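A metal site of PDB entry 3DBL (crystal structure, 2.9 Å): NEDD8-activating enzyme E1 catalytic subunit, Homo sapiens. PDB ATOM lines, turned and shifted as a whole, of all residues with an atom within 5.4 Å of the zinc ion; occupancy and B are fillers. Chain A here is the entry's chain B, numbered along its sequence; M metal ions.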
ATOM      1  N   ILE A 151       1.743 -10.090  -8.717  1.00  0.00           N
ATOM      2  CA  ILE A 151       0.608  -9.723  -7.884  1.00  0.00           C
ATOM      3  C   ILE A 151      -0.548  -9.310  -8.784  1.00  0.00           C
ATOM      4  O   ILE A 151      -1.717  -9.488  -8.427  1.00  0.00           O
ATOM      5  CB  ILE A 151       1.004  -8.575  -6.911  1.00  0.00           C
ATOM      6  CG1 ILE A 151       1.579  -9.169  -5.638  1.00  0.00           C
ATOM      7  CG2 ILE A 151      -0.202  -7.717  -6.565  1.00  0.00           C
ATOM      8  CD1 ILE A 151       2.191  -8.146  -4.704  1.00  0.00           C
ATOM      9  N   ALA A 190       3.784 -12.207   2.811  1.00  0.00           N
ATOM     10  CA  ALA A 190       4.327 -10.852   2.754  1.00  0.00           C
ATOM     11  C   ALA A 190       5.133 -10.773   1.453  1.00  0.00           C
ATOM     12  O   ALA A 190       5.893 -11.698   1.143  1.00  0.00           O
ATOM     13  CB  ALA A 190       5.250 -10.605   3.954  1.00  0.00           C
ATOM     14  N   CYS A 191       4.970  -9.692   0.703  1.00  0.00           N
ATOM     15  CA  CYS A 191       5.692  -9.534  -0.559  1.00  0.00           C
ATOM     16  C   CYS A 191       6.863  -8.550  -0.426  1.00  0.00           C
ATOM     17  O   CYS A 191       7.090  -7.996   0.653  1.00  0.00           O
ATOM     18  CB  CYS A 191       4.736  -9.025  -1.643  1.00  0.00           C
ATOM     19  SG  CYS A 191       4.238  -7.285  -1.424  1.00  0.00           S
ATOM     20  N   GLU A 193       7.255  -5.448  -1.367  1.00  0.00           N
ATOM     21  CA  GLU A 193       6.858  -4.138  -0.861  1.00  0.00           C
ATOM     22  C   GLU A 193       6.527  -4.228   0.627  1.00  0.00           C
ATOM     23  O   GLU A 193       6.798  -3.308   1.379  1.00  0.00           O
ATOM     24  CB  GLU A 193       5.636  -3.594  -1.611  1.00  0.00           C
ATOM     25  CG  GLU A 193       5.863  -3.251  -3.095  1.00  0.00           C
ATOM     26  CD  GLU A 193       6.956  -2.207  -3.324  1.00  0.00           C
ATOM     27  OE1 GLU A 193       7.005  -1.211  -2.567  1.00  0.00           O
ATOM     28  OE2 GLU A 193       7.757  -2.365  -4.276  1.00  0.00           O
ATOM     29  N   CYS A 194       5.956  -5.354   1.042  1.00  0.00           N
ATOM     30  CA  CYS A 194       5.600  -5.568   2.448  1.00  0.00           C
ATOM     31  C   CYS A 194       6.806  -5.396   3.342  1.00  0.00           C
ATOM     32  O   CYS A 194       6.677  -5.087   4.529  1.00  0.00           O
ATOM     33  CB  CYS A 194       5.070  -6.983   2.670  1.00  0.00           C
ATOM     34  SG  CYS A 194       3.283  -7.208   2.511  1.00  0.00           S
ATOM     35  N   ARG A 331       2.738  -9.989   6.808  1.00  0.00           N
ATOM     36  CA  ARG A 331       2.246  -9.314   5.616  1.00  0.00           C
ATOM     37  C   ARG A 331       1.618  -7.985   6.014  1.00  0.00           C
ATOM     38  O   ARG A 331       0.513  -7.962   6.527  1.00  0.00           O
ATOM     39  CB  ARG A 331       1.213 -10.200   4.919  1.00  0.00           C
ATOM     40  CG  ARG A 331       0.360  -9.475   3.906  1.00  0.00           C
ATOM     41  CD  ARG A 331      -0.635 -10.423   3.239  1.00  0.00           C
ATOM     42  NE  ARG A 331      -1.484  -9.718   2.295  1.00  0.00           N
ATOM     43  CZ  ARG A 331      -2.251 -10.311   1.397  1.00  0.00           C
ATOM     44  NH1 ARG A 331      -2.263 -11.638   1.317  1.00  0.00           N
ATOM     45  NH2 ARG A 331      -2.992  -9.596   0.550  1.00  0.00           N
ATOM     46  N   LYS A 332       2.329  -6.878   5.796  1.00  0.00           N
ATOM     47  CA  LYS A 332       1.795  -5.550   6.119  1.00  0.00           C
ATOM     48  C   LYS A 332       0.381  -5.441   5.527  1.00  0.00           C
ATOM     49  O   LYS A 332       0.201  -5.471   4.312  1.00  0.00           O
ATOM     50  CB  LYS A 332       2.753  -4.499   5.553  1.00  0.00           C
ATOM     51  CG  LYS A 332       2.292  -3.052   5.674  1.00  0.00           C
ATOM     52  CD  LYS A 332       3.466  -2.037   5.637  1.00  0.00           C
ATOM     53  CE  LYS A 332       4.287  -2.084   6.937  1.00  0.00           C
ATOM     54  NZ  LYS A 332       5.260  -0.953   7.065  1.00  0.00           N
ATOM     55  N   CYS A 335      -0.541  -2.819   2.706  1.00  0.00           N
ATOM     56  CA  CYS A 335       0.469  -2.781   1.667  1.00  0.00           C
ATOM     57  C   CYS A 335      -0.043  -2.137   0.395  1.00  0.00           C
ATOM     58  O   CYS A 335      -1.087  -2.502  -0.124  1.00  0.00           O
ATOM     59  CB  CYS A 335       0.946  -4.201   1.337  1.00  0.00           C
ATOM     60  SG  CYS A 335       2.275  -4.190   0.136  1.00  0.00           S
ATOM     61  N   ALA A 337       0.985  -2.607  -2.319  1.00  0.00           N
ATOM     62  CA  ALA A 337       1.186  -3.590  -3.373  1.00  0.00           C
ATOM     63  C   ALA A 337       0.171  -4.730  -3.343  1.00  0.00           C
ATOM     64  O   ALA A 337      -0.682  -4.811  -4.218  1.00  0.00           O
ATOM     65  CB  ALA A 337       2.601  -4.147  -3.296  1.00  0.00           C
ATOM     66  N   CYS A 338       0.261  -5.604  -2.347  1.00  0.00           N
ATOM     67  CA  CYS A 338      -0.640  -6.749  -2.258  1.00  0.00           C
ATOM     68  C   CYS A 338      -1.949  -6.518  -1.510  1.00  0.00           C
ATOM     69  O   CYS A 338      -2.542  -7.443  -0.975  1.00  0.00           O
ATOM     70  CB  CYS A 338       0.090  -7.933  -1.623  1.00  0.00           C
ATOM     71  SG  CYS A 338       0.491  -7.724   0.107  1.00  0.00           S
HETATM   72 ZN    ZN M   1       2.604  -6.475   0.267  1.00  0.00          ZN
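The zinc ion is bound by the side-chain sulfur (SG) of Cys 335, the side-chain sulfur (SG) of Cys 194, the side-chain sulfur (SG) of Cys 338 and the side-chain sulfur (SG) of Cys 191.
The side-chain sulfur of Cys 335 sits close to the backbone NH of Ala 337 (3.2 Å). The side-chain sulfur of Cys 194 lies close to the backbone NH of Lys 332 (3.4 Å). The guanidinium group of Arg 331 sits at hydrogen-bond distance from the backbone carbonyl oxygen of Cys 338 (2.7 Å). The backbone NH of Glu 193 sits close to the side-chain sulfur of Cys 191 (3.5 Å).
Within 4 Å of the zinc ion: Cys 191, Cys 194, Cys 335 and Cys 338. Along chain A the residues within 4 Å of the zinc ion span positions 191 to 338.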
